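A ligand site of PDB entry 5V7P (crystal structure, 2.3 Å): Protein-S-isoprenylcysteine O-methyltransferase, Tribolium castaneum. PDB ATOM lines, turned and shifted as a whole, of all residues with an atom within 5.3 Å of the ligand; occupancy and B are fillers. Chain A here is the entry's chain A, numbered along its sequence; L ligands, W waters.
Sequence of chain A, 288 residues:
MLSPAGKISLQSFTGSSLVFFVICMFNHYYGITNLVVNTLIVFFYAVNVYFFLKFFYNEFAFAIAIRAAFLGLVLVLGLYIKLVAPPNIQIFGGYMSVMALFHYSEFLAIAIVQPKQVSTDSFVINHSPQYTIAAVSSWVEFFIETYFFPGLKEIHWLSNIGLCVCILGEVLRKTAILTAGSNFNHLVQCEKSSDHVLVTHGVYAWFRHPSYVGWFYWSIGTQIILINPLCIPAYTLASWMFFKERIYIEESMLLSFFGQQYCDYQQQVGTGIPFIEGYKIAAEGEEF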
ATOM      1  N   ALA A 176     -19.606  22.531  -0.368  1.00  0.00           N
ATOM      2  CA  ALA A 176     -18.901  22.127   0.858  1.00  0.00           C
ATOM      3  C   ALA A 176     -19.872  22.001   2.022  1.00  0.00           C
ATOM      4  O   ALA A 176     -19.809  21.028   2.783  1.00  0.00           O
ATOM      5  CB  ALA A 176     -17.796  23.135   1.175  1.00  0.00           C
ATOM      6  N   ASN A 183     -21.789  18.326  10.057  1.00  0.00           N
ATOM      7  CA  ASN A 183     -20.428  18.619  10.509  1.00  0.00           C
ATOM      8  C   ASN A 183     -20.024  20.053  10.203  1.00  0.00           C
ATOM      9  O   ASN A 183     -19.009  20.520  10.753  1.00  0.00           O
ATOM     10  CB  ASN A 183     -19.432  17.662   9.850  1.00  0.00           C
ATOM     11  CG  ASN A 183     -19.821  16.209  10.028  1.00  0.00           C
ATOM     12  OD1 ASN A 183     -19.645  15.632  11.098  1.00  0.00           O
ATOM     13  ND2 ASN A 183     -20.348  15.596   8.965  1.00  0.00           N
ATOM     14  N   PHE A 184     -20.759  20.763   9.356  1.00  0.00           N
ATOM     15  CA  PHE A 184     -20.502  22.173   9.111  1.00  0.00           C
ATOM     16  C   PHE A 184     -21.067  23.002  10.248  1.00  0.00           C
ATOM     17  O   PHE A 184     -21.994  22.599  10.945  1.00  0.00           O
ATOM     18  CB  PHE A 184     -21.123  22.612   7.785  1.00  0.00           C
ATOM     19  CG  PHE A 184     -20.681  23.978   7.329  1.00  0.00           C
ATOM     20  CD1 PHE A 184     -19.518  24.152   6.597  1.00  0.00           C
ATOM     21  CD2 PHE A 184     -21.436  25.101   7.632  1.00  0.00           C
ATOM     22  CE1 PHE A 184     -19.112  25.401   6.187  1.00  0.00           C
ATOM     23  CE2 PHE A 184     -21.039  26.359   7.229  1.00  0.00           C
ATOM     24  CZ  PHE A 184     -19.878  26.510   6.495  1.00  0.00           C
ATOM     25  N   ASN A 185     -20.494  24.188  10.439  1.00  0.00           N
ATOM     26  CA  ASN A 185     -20.981  25.114  11.457  1.00  0.00           C
ATOM     27  C   ASN A 185     -20.408  26.483  11.173  1.00  0.00           C
ATOM     28  O   ASN A 185     -19.209  26.622  10.913  1.00  0.00           O
ATOM     29  CB  ASN A 185     -20.587  24.644  12.855  1.00  0.00           C
ATOM     30  CG  ASN A 185     -21.476  25.229  13.938  1.00  0.00           C
ATOM     31  OD1 ASN A 185     -21.803  26.417  13.922  1.00  0.00           O
ATOM     32  ND2 ASN A 185     -21.874  24.394  14.887  1.00  0.00           N
ATOM     33  N   HIS A 186     -21.273  27.504  11.207  1.00  0.00           N
ATOM     34  CA  HIS A 186     -20.797  28.883  11.051  1.00  0.00           C
ATOM     35  C   HIS A 186     -19.850  29.282  12.175  1.00  0.00           C
ATOM     36  O   HIS A 186     -19.040  30.193  11.997  1.00  0.00           O
ATOM     37  CB  HIS A 186     -21.988  29.846  11.016  1.00  0.00           C
ATOM     38  CG  HIS A 186     -22.558  30.036   9.640  1.00  0.00           C
ATOM     39  ND1 HIS A 186     -23.898  30.308   9.420  1.00  0.00           N
ATOM     40  CD2 HIS A 186     -21.984  29.994   8.412  1.00  0.00           C
ATOM     41  CE1 HIS A 186     -24.112  30.434   8.130  1.00  0.00           C
ATOM     42  NE2 HIS A 186     -22.976  30.246   7.493  1.00  0.00           N
ATOM     43  N   LEU A 187     -19.929  28.605  13.324  1.00  0.00           N
ATOM     44  CA  LEU A 187     -19.065  28.868  14.461  1.00  0.00           C
ATOM     45  C   LEU A 187     -18.080  27.726  14.630  1.00  0.00           C
ATOM     46  O   LEU A 187     -18.480  26.555  14.640  1.00  0.00           O
ATOM     47  CB  LEU A 187     -19.893  29.042  15.735  1.00  0.00           C
ATOM     48  CG  LEU A 187     -20.474  30.428  16.005  1.00  0.00           C
ATOM     49  CD1 LEU A 187     -21.160  31.015  14.786  1.00  0.00           C
ATOM     50  CD2 LEU A 187     -21.448  30.369  17.176  1.00  0.00           C
ATOM     51  N   VAL A 188     -16.792  28.064  14.736  1.00  0.00           N
ATOM     52  CA  VAL A 188     -15.777  27.054  14.973  1.00  0.00           C
ATOM     53  C   VAL A 188     -16.049  26.369  16.303  1.00  0.00           C
ATOM     54  O   VAL A 188     -16.332  27.010  17.324  1.00  0.00           O
ATOM     55  CB  VAL A 188     -14.373  27.679  14.946  1.00  0.00           C
ATOM     56  CG1 VAL A 188     -13.300  26.645  15.284  1.00  0.00           C
ATOM     57  CG2 VAL A 188     -14.104  28.288  13.570  1.00  0.00           C
ATOM     58  N   GLN A 189     -15.950  25.035  16.309  1.00  0.00           N
ATOM     59  CA  GLN A 189     -16.241  24.225  17.479  1.00  0.00           C
ATOM     60  C   GLN A 189     -14.951  23.854  18.183  1.00  0.00           C
ATOM     61  O   GLN A 189     -13.994  23.406  17.534  1.00  0.00           O
ATOM     62  CB  GLN A 189     -17.015  22.969  17.089  1.00  0.00           C
ATOM     63  CG  GLN A 189     -18.310  23.235  16.345  1.00  0.00           C
ATOM     64  CD  GLN A 189     -19.305  24.010  17.185  1.00  0.00           C
ATOM     65  OE1 GLN A 189     -19.781  23.530  18.215  1.00  0.00           O
ATOM     66  NE2 GLN A 189     -19.636  25.211  16.742  1.00  0.00           N
ATOM     67  N   HIS A 196     -19.946  14.178  15.472  1.00  0.00           N
ATOM     68  CA  HIS A 196     -19.030  14.884  14.575  1.00  0.00           C
ATOM     69  C   HIS A 196     -18.028  13.902  13.994  1.00  0.00           C
ATOM     70  O   HIS A 196     -17.266  13.261  14.741  1.00  0.00           O
ATOM     71  CB  HIS A 196     -18.332  16.009  15.334  1.00  0.00           C
ATOM     72  CG  HIS A 196     -17.554  16.940  14.453  1.00  0.00           C
ATOM     73  ND1 HIS A 196     -16.830  17.999  14.947  1.00  0.00           N
ATOM     74  CD2 HIS A 196     -17.399  16.967  13.110  1.00  0.00           C
ATOM     75  CE1 HIS A 196     -16.263  18.642  13.956  1.00  0.00           C
ATOM     76  NE2 HIS A 196     -16.584  18.035  12.829  1.00  0.00           N
ATOM     77  N   VAL A 197     -18.019  13.776  12.669  1.00  0.00           N
ATOM     78  CA  VAL A 197     -17.123  12.855  11.978  1.00  0.00           C
ATOM     79  C   VAL A 197     -16.266  13.655  11.000  1.00  0.00           C
ATOM     80  O   VAL A 197     -16.599  14.776  10.613  1.00  0.00           O
ATOM     81  CB  VAL A 197     -17.898  11.742  11.240  1.00  0.00           C
ATOM     82  CG1 VAL A 197     -18.658  10.880  12.234  1.00  0.00           C
ATOM     83  CG2 VAL A 197     -18.848  12.333  10.200  1.00  0.00           C
ATOM     84  N   LEU A 198     -15.156  13.048  10.611  1.00  0.00           N
ATOM     85  CA  LEU A 198     -14.242  13.676   9.666  1.00  0.00           C
ATOM     86  C   LEU A 198     -14.737  13.469   8.241  1.00  0.00           C
ATOM     87  O   LEU A 198     -15.149  12.372   7.863  1.00  0.00           O
ATOM     88  CB  LEU A 198     -12.826  13.115   9.834  1.00  0.00           C
ATOM     89  CG  LEU A 198     -11.760  13.665   8.881  1.00  0.00           C
ATOM     90  CD1 LEU A 198     -11.647  15.178   8.989  1.00  0.00           C
ATOM     91  CD2 LEU A 198     -10.422  12.999   9.164  1.00  0.00           C
ATOM     92  N   VAL A 199     -14.671  14.542   7.455  1.00  0.00           N
ATOM     93  CA  VAL A 199     -15.129  14.554   6.070  1.00  0.00           C
ATOM     94  C   VAL A 199     -13.903  14.714   5.187  1.00  0.00           C
ATOM     95  O   VAL A 199     -13.164  15.697   5.316  1.00  0.00           O
ATOM     96  CB  VAL A 199     -16.144  15.678   5.821  1.00  0.00           C
ATOM     97  CG1 VAL A 199     -16.632  15.661   4.373  1.00  0.00           C
ATOM     98  CG2 VAL A 199     -17.317  15.568   6.781  1.00  0.00           C
ATOM     99  N   TYR A 204     -13.985  18.134  -0.190  1.00  0.00           N
ATOM    100  CA  TYR A 204     -13.018  17.975   0.894  1.00  0.00           C
ATOM    101  C   TYR A 204     -11.857  17.069   0.495  1.00  0.00           C
ATOM    102  O   TYR A 204     -10.867  16.994   1.241  1.00  0.00           O
ATOM    103  CB  TYR A 204     -13.707  17.441   2.147  1.00  0.00           C
ATOM    104  CG  TYR A 204     -14.496  18.516   2.846  1.00  0.00           C
ATOM    105  CD1 TYR A 204     -15.830  18.756   2.523  1.00  0.00           C
ATOM    106  CD2 TYR A 204     -13.909  19.320   3.812  1.00  0.00           C
ATOM    107  CE1 TYR A 204     -16.552  19.753   3.159  1.00  0.00           C
ATOM    108  CE2 TYR A 204     -14.622  20.316   4.447  1.00  0.00           C
ATOM    109  CZ  TYR A 204     -15.939  20.523   4.115  1.00  0.00           C
ATOM    110  OH  TYR A 204     -16.652  21.518   4.750  1.00  0.00           O
ATOM    111  N   ARG A 208      -8.816  21.134   2.184  1.00  0.00           N
ATOM    112  CA  ARG A 208      -9.211  20.887   3.566  1.00  0.00           C
ATOM    113  C   ARG A 208     -10.264  21.864   4.051  1.00  0.00           C
ATOM    114  O   ARG A 208     -10.994  21.550   4.995  1.00  0.00           O
ATOM    115  CB  ARG A 208      -7.987  20.939   4.486  1.00  0.00           C
ATOM    116  CG  ARG A 208      -6.892  19.956   4.114  1.00  0.00           C
ATOM    117  CD  ARG A 208      -6.122  19.496   5.337  1.00  0.00           C
ATOM    118  NE  ARG A 208      -5.426  20.592   6.008  1.00  0.00           N
ATOM    119  CZ  ARG A 208      -4.191  20.995   5.733  1.00  0.00           C
ATOM    120  NH1 ARG A 208      -3.482  20.410   4.776  1.00  0.00           N
ATOM    121  NH2 ARG A 208      -3.655  22.009   6.408  1.00  0.00           N
ATOM    122  N   HIS A 209     -10.363  23.041   3.431  1.00  0.00           N
ATOM    123  CA  HIS A 209     -11.306  24.080   3.844  1.00  0.00           C
ATOM    124  C   HIS A 209     -11.996  24.655   2.606  1.00  0.00           C
ATOM    125  O   HIS A 209     -11.877  25.845   2.313  1.00  0.00           O
ATOM    126  CB  HIS A 209     -10.588  25.168   4.639  1.00  0.00           C
ATOM    127  CG  HIS A 209      -9.738  24.623   5.747  1.00  0.00           C
ATOM    128  ND1 HIS A 209     -10.254  24.170   6.937  1.00  0.00           N
ATOM    129  CD2 HIS A 209      -8.393  24.447   5.827  1.00  0.00           C
ATOM    130  CE1 HIS A 209      -9.275  23.746   7.714  1.00  0.00           C
ATOM    131  NE2 HIS A 209      -8.136  23.897   7.064  1.00  0.00           N
ATOM    132  N   PRO A 210     -12.751  23.827   1.879  1.00  0.00           N
ATOM    133  CA  PRO A 210     -13.350  24.312   0.628  1.00  0.00           C
ATOM    134  C   PRO A 210     -14.348  25.447   0.821  1.00  0.00           C
ATOM    135  O   PRO A 210     -14.513  26.273  -0.097  1.00  0.00           O
ATOM    136  CB  PRO A 210     -14.031  23.057   0.057  1.00  0.00           C
ATOM    137  CG  PRO A 210     -14.275  22.190   1.250  1.00  0.00           C
ATOM    138  CD  PRO A 210     -13.132  22.440   2.179  1.00  0.00           C
ATOM    139  N   SER A 211     -15.028  25.522   1.967  1.00  0.00           N
ATOM    140  CA  SER A 211     -15.956  26.621   2.181  1.00  0.00           C
ATOM    141  C   SER A 211     -15.219  27.938   2.364  1.00  0.00           C
ATOM    142  O   SER A 211     -15.686  28.987   1.916  1.00  0.00           O
ATOM    143  CB  SER A 211     -16.859  26.331   3.382  1.00  0.00           C
ATOM    144  OG  SER A 211     -16.288  26.823   4.592  1.00  0.00           O
ATOM    145  N   TYR A 212     -14.043  27.916   2.993  1.00  0.00           N
ATOM    146  CA  TYR A 212     -13.233  29.123   3.105  1.00  0.00           C
ATOM    147  C   TYR A 212     -12.590  29.479   1.768  1.00  0.00           C
ATOM    148  O   TYR A 212     -12.411  30.671   1.474  1.00  0.00           O
ATOM    149  CB  TYR A 212     -12.166  28.962   4.183  1.00  0.00           C
ATOM    150  CG  TYR A 212     -12.715  28.677   5.572  1.00  0.00           C
ATOM    151  CD1 TYR A 212     -14.038  28.948   5.891  1.00  0.00           C
ATOM    152  CD2 TYR A 212     -11.908  28.133   6.554  1.00  0.00           C
ATOM    153  CE1 TYR A 212     -14.538  28.686   7.151  1.00  0.00           C
ATOM    154  CE2 TYR A 212     -12.396  27.873   7.826  1.00  0.00           C
ATOM    155  CZ  TYR A 212     -13.712  28.151   8.114  1.00  0.00           C
ATOM    156  OH  TYR A 212     -14.212  27.889   9.374  1.00  0.00           O
ATOM    157  N   VAL A 213     -12.240  28.483   0.960  1.00  0.00           N
ATOM    158  CA  VAL A 213     -11.706  28.761  -0.374  1.00  0.00           C
ATOM    159  C   VAL A 213     -12.751  29.490  -1.207  1.00  0.00           C
ATOM    160  O   VAL A 213     -12.462  30.513  -1.834  1.00  0.00           O
ATOM    161  CB  VAL A 213     -11.263  27.447  -1.053  1.00  0.00           C
ATOM    162  CG1 VAL A 213     -10.843  27.706  -2.500  1.00  0.00           C
ATOM    163  CG2 VAL A 213     -10.125  26.803  -0.289  1.00  0.00           C
ATOM    164  N   GLU A 250      -8.664  26.424  14.028  1.00  0.00           N
ATOM    165  CA  GLU A 250      -9.671  25.421  13.675  1.00  0.00           C
ATOM    166  C   GLU A 250      -9.056  24.043  13.537  1.00  0.00           C
ATOM    167  O   GLU A 250      -9.635  23.041  13.978  1.00  0.00           O
ATOM    168  CB  GLU A 250     -10.391  25.841  12.389  1.00  0.00           C
ATOM    169  CG  GLU A 250     -11.412  24.847  11.889  1.00  0.00           C
ATOM    170  CD  GLU A 250     -12.315  25.436  10.822  1.00  0.00           C
ATOM    171  OE1 GLU A 250     -12.504  26.675  10.820  1.00  0.00           O
ATOM    172  OE2 GLU A 250     -12.834  24.678   9.975  1.00  0.00           O
ATOM    173  N   LEU A 254      -9.385  20.269  15.346  1.00  0.00           N
ATOM    174  CA  LEU A 254      -9.628  19.074  14.559  1.00  0.00           C
ATOM    175  C   LEU A 254      -8.613  17.980  14.874  1.00  0.00           C
ATOM    176  O   LEU A 254      -8.959  16.798  14.828  1.00  0.00           O
ATOM    177  CB  LEU A 254      -9.600  19.416  13.063  1.00  0.00           C
ATOM    178  CG  LEU A 254     -10.810  20.191  12.548  1.00  0.00           C
ATOM    179  CD1 LEU A 254     -10.510  20.851  11.213  1.00  0.00           C
ATOM    180  CD2 LEU A 254     -12.025  19.282  12.426  1.00  0.00           C
ATOM    181  N   PHE A 257      -9.741  16.319  17.837  1.00  0.00           N
ATOM    182  CA  PHE A 257     -10.949  15.553  17.556  1.00  0.00           C
ATOM    183  C   PHE A 257     -10.615  14.201  16.929  1.00  0.00           C
ATOM    184  O   PHE A 257     -11.084  13.156  17.409  1.00  0.00           O
ATOM    185  CB  PHE A 257     -11.878  16.336  16.622  1.00  0.00           C
ATOM    186  CG  PHE A 257     -12.467  17.587  17.233  1.00  0.00           C
ATOM    187  CD1 PHE A 257     -12.285  17.884  18.574  1.00  0.00           C
ATOM    188  CD2 PHE A 257     -13.199  18.458  16.451  1.00  0.00           C
ATOM    189  CE1 PHE A 257     -12.839  19.037  19.123  1.00  0.00           C
ATOM    190  CE2 PHE A 257     -13.745  19.606  16.985  1.00  0.00           C
ATOM    191  CZ  PHE A 257     -13.565  19.896  18.321  1.00  0.00           C
ATOM    192  N   PHE A 258      -9.818  14.202  15.860  1.00  0.00           N
ATOM    193  CA  PHE A 258      -9.608  13.019  15.048  1.00  0.00           C
ATOM    194  C   PHE A 258      -8.162  12.542  15.032  1.00  0.00           C
ATOM    195  O   PHE A 258      -7.857  11.559  14.351  1.00  0.00           O
ATOM    196  CB  PHE A 258     -10.086  13.284  13.621  1.00  0.00           C
ATOM    197  CG  PHE A 258     -11.471  13.857  13.541  1.00  0.00           C
ATOM    198  CD1 PHE A 258     -12.577  13.075  13.858  1.00  0.00           C
ATOM    199  CD2 PHE A 258     -11.682  15.169  13.174  1.00  0.00           C
ATOM    200  CE1 PHE A 258     -13.856  13.599  13.791  1.00  0.00           C
ATOM    201  CE2 PHE A 258     -12.960  15.694  13.106  1.00  0.00           C
ATOM    202  CZ  PHE A 258     -14.047  14.915  13.413  1.00  0.00           C
ATOM    203  N   TYR A 262      -6.741  13.184  11.025  1.00  0.00           N
ATOM    204  CA  TYR A 262      -6.577  14.513  10.452  1.00  0.00           C
ATOM    205  C   TYR A 262      -5.122  14.786  10.099  1.00  0.00           C
ATOM    206  O   TYR A 262      -4.850  15.500   9.128  1.00  0.00           O
ATOM    207  CB  TYR A 262      -7.086  15.587  11.409  1.00  0.00           C
ATOM    208  CG  TYR A 262      -7.365  16.886  10.695  1.00  0.00           C
ATOM    209  CD1 TYR A 262      -8.535  17.060   9.971  1.00  0.00           C
ATOM    210  CD2 TYR A 262      -6.450  17.931  10.713  1.00  0.00           C
ATOM    211  CE1 TYR A 262      -8.801  18.231   9.307  1.00  0.00           C
ATOM    212  CE2 TYR A 262      -6.704  19.115  10.045  1.00  0.00           C
ATOM    213  CZ  TYR A 262      -7.886  19.258   9.337  1.00  0.00           C
ATOM    214  OH  TYR A 262      -8.162  20.430   8.675  1.00  0.00           O
ATOM    215  N   TYR A 265      -4.737  13.454   6.869  1.00  0.00           N
ATOM    216  CA  TYR A 265      -5.498  14.300   5.943  1.00  0.00           C
ATOM    217  C   TYR A 265      -4.712  15.562   5.583  1.00  0.00           C
ATOM    218  O   TYR A 265      -4.833  16.048   4.454  1.00  0.00           O
ATOM    219  CB  TYR A 265      -6.840  14.650   6.583  1.00  0.00           C
ATOM    220  CG  TYR A 265      -7.776  15.477   5.734  1.00  0.00           C
ATOM    221  CD1 TYR A 265      -8.070  15.130   4.426  1.00  0.00           C
ATOM    222  CD2 TYR A 265      -8.395  16.602   6.269  1.00  0.00           C
ATOM    223  CE1 TYR A 265      -8.944  15.885   3.660  1.00  0.00           C
ATOM    224  CE2 TYR A 265      -9.258  17.364   5.507  1.00  0.00           C
ATOM    225  CZ  TYR A 265      -9.532  17.004   4.214  1.00  0.00           C
ATOM    226  OH  TYR A 265     -10.402  17.765   3.475  1.00  0.00           O
HETATM  227  N1  LIG L   1     -13.149  24.661   7.378  1.00  0.00           N
HETATM  228  C1  LIG L   1     -14.160  23.886   6.672  1.00  0.00           C
HETATM  229  C2  LIG L   1     -15.472  23.878   7.465  1.00  0.00           C
HETATM  230  C3  LIG L   1     -15.955  25.253   7.901  1.00  0.00           C
HETATM  231  S1  LIG L   1     -17.366  25.110   9.038  1.00  0.00           S
HETATM  232  C4  LIG L   1     -14.403  24.448   5.276  1.00  0.00           C
HETATM  233  O1  LIG L   1     -13.991  25.572   4.954  1.00  0.00           O
HETATM  234  O2  LIG L   1     -15.012  23.804   4.422  1.00  0.00           O
HETATM  235  C5  LIG L   1     -16.336  25.026  10.542  1.00  0.00           C
HETATM  236  C6  LIG L   1     -16.516  23.726  11.323  1.00  0.00           C
HETATM  237  O3  LIG L   1     -16.291  22.616  10.485  1.00  0.00           O
HETATM  238  C7  LIG L   1     -15.513  23.653  12.469  1.00  0.00           C
HETATM  239  O4  LIG L   1     -16.184  23.529  13.704  1.00  0.00           O
HETATM  240  C8  LIG L   1     -14.665  22.433  12.184  1.00  0.00           C
HETATM  241  O5  LIG L   1     -14.487  21.662  13.358  1.00  0.00           O
HETATM  242  C9  LIG L   1     -15.430  21.681  11.104  1.00  0.00           C
HETATM  243  N2  LIG L   1     -14.559  21.056  10.092  1.00  0.00           N
HETATM  244  C10 LIG L   1     -13.512  21.635   9.404  1.00  0.00           C
HETATM  245  N3  LIG L   1     -12.985  20.726   8.561  1.00  0.00           N
HETATM  246  C11 LIG L   1     -13.684  19.569   8.687  1.00  0.00           C
HETATM  247  C12 LIG L   1     -13.561  18.335   8.059  1.00  0.00           C
HETATM  248  N4  LIG L   1     -12.627  18.123   7.146  1.00  0.00           N
HETATM  249  N5  LIG L   1     -14.433  17.331   8.406  1.00  0.00           N
HETATM  250  C13 LIG L   1     -15.412  17.549   9.359  1.00  0.00           C
HETATM  251  N6  LIG L   1     -15.517  18.772   9.980  1.00  0.00           N
HETATM  252  C14 LIG L   1     -14.665  19.764   9.638  1.00  0.00           C
HETATM  253  O   HOH W   1     -17.351  28.374   9.716  1.00  0.00           O
HETATM  254  O   HOH W   2     -17.973  21.235  13.292  1.00  0.00           O
HETATM  255  O   HOH W   3     -12.862  23.006  14.943  1.00  0.00           O
HETATM  256  O   HOH W   4     -10.668  20.322   7.339  1.00  0.00           O
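N1 of the ligand lies within salt-bridge range of OE2 of Glu 250, 2.6 Å away. An oxygen (O2) of the ligand is in hydrogen-bond range of the backbone NH of Ser 211 (3.0 Å). An oxygen (O1) of the ligand sits at hydrogen-bond distance from the side-chain hydroxyl of Ser 211 (2.6 Å). An oxygen (O2) of the ligand lies within hydrogen-bond range of the side-chain hydroxyl (OH) of Tyr 204 (2.8 Å). A nitrogen (N5) of the ligand lies within hydrogen-bond range of the backbone NH of Val 199, 3.0 Å away. O of Val 199 is in hydrogen-bond range of N4 of the ligand (3.1 Å). ND1 of His 209 lies within hydrogen-bond range of N1 of the ligand, 3.0 Å away. N of Gln 189 sits at hydrogen-bond distance from O4 of the ligand. N of Asn 185 sits close to S1 of the ligand (3.5 Å). The backbone NH (N) of Tyr 212 lies within hydrogen-bond range of an oxygen (O1) of the ligand, at 3.1 Å. N6 of the ligand lies within hydrogen-bond range of NE2 of His 196, at 3.1 Å.
OE1 of Glu 250 lies within hydrogen-bond range of OH of Tyr 212 (2.5 Å). O of Tyr 204 sits at hydrogen-bond distance from OH of Tyr 265, 2.4 Å away. NE2 of Gln 189 lies close to ND2 of Asn 185, 3.0 Å away. The backbone carbonyl oxygen (O) of Leu 187 lies within hydrogen-bond range of the side-chain amide nitrogen (NE2) of Gln 189 (2.7 Å). The backbone NH (N) of Leu 187 is in hydrogen-bond range of the side-chain amide oxygen (OD1) of Asn 185, at 2.9 Å. The backbone NH of Val 197 lies within hydrogen-bond range of the side-chain amide oxygen of Asn 183 (2.9 Å).
The backbone carbonyl oxygen (O) of Asn 183 lies close to an oxygen (O3) of the ligand (3.4 Å). N of Pro 210 lies close to O2 of the ligand. CE1 of Phe 184 touches S1 of the ligand, at 3.4 Å. Leu 187 touches the ligand (O to O4, 3.9 Å). Val 188 touches the ligand. Val 197 touches the ligand. Leu 198 touches the ligand. CD2 of Leu 254 touches O5 of the ligand (3.5 Å). Tyr 265 touches the ligand (CE2 to N4, 3.8 Å). Within 4 Å of the ligand: Asn 183, Phe 184, Asn 185, Leu 187, Val 188, Gln 189, His 196, Val 197, Leu 198, Val 199, Tyr 204, His 209, Pro 210, Ser 211, Tyr 212, Glu 250, Leu 254 and Tyr 265.
Water W3 lies within hydrogen-bond range of O5 of the ligand (2.6 Å), O of Gln 189 (2.9 Å) and O of Glu 250 (3.4 Å). Water W4 lies within hydrogen-bond range of N3 of the ligand, O of Arg 208 and OH of Tyr 262. Water W2 bridges the backbone carbonyl oxygen (O) of Asn 183 (2.8 Å) and an oxygen (O4) of the ligand (2.9 Å).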
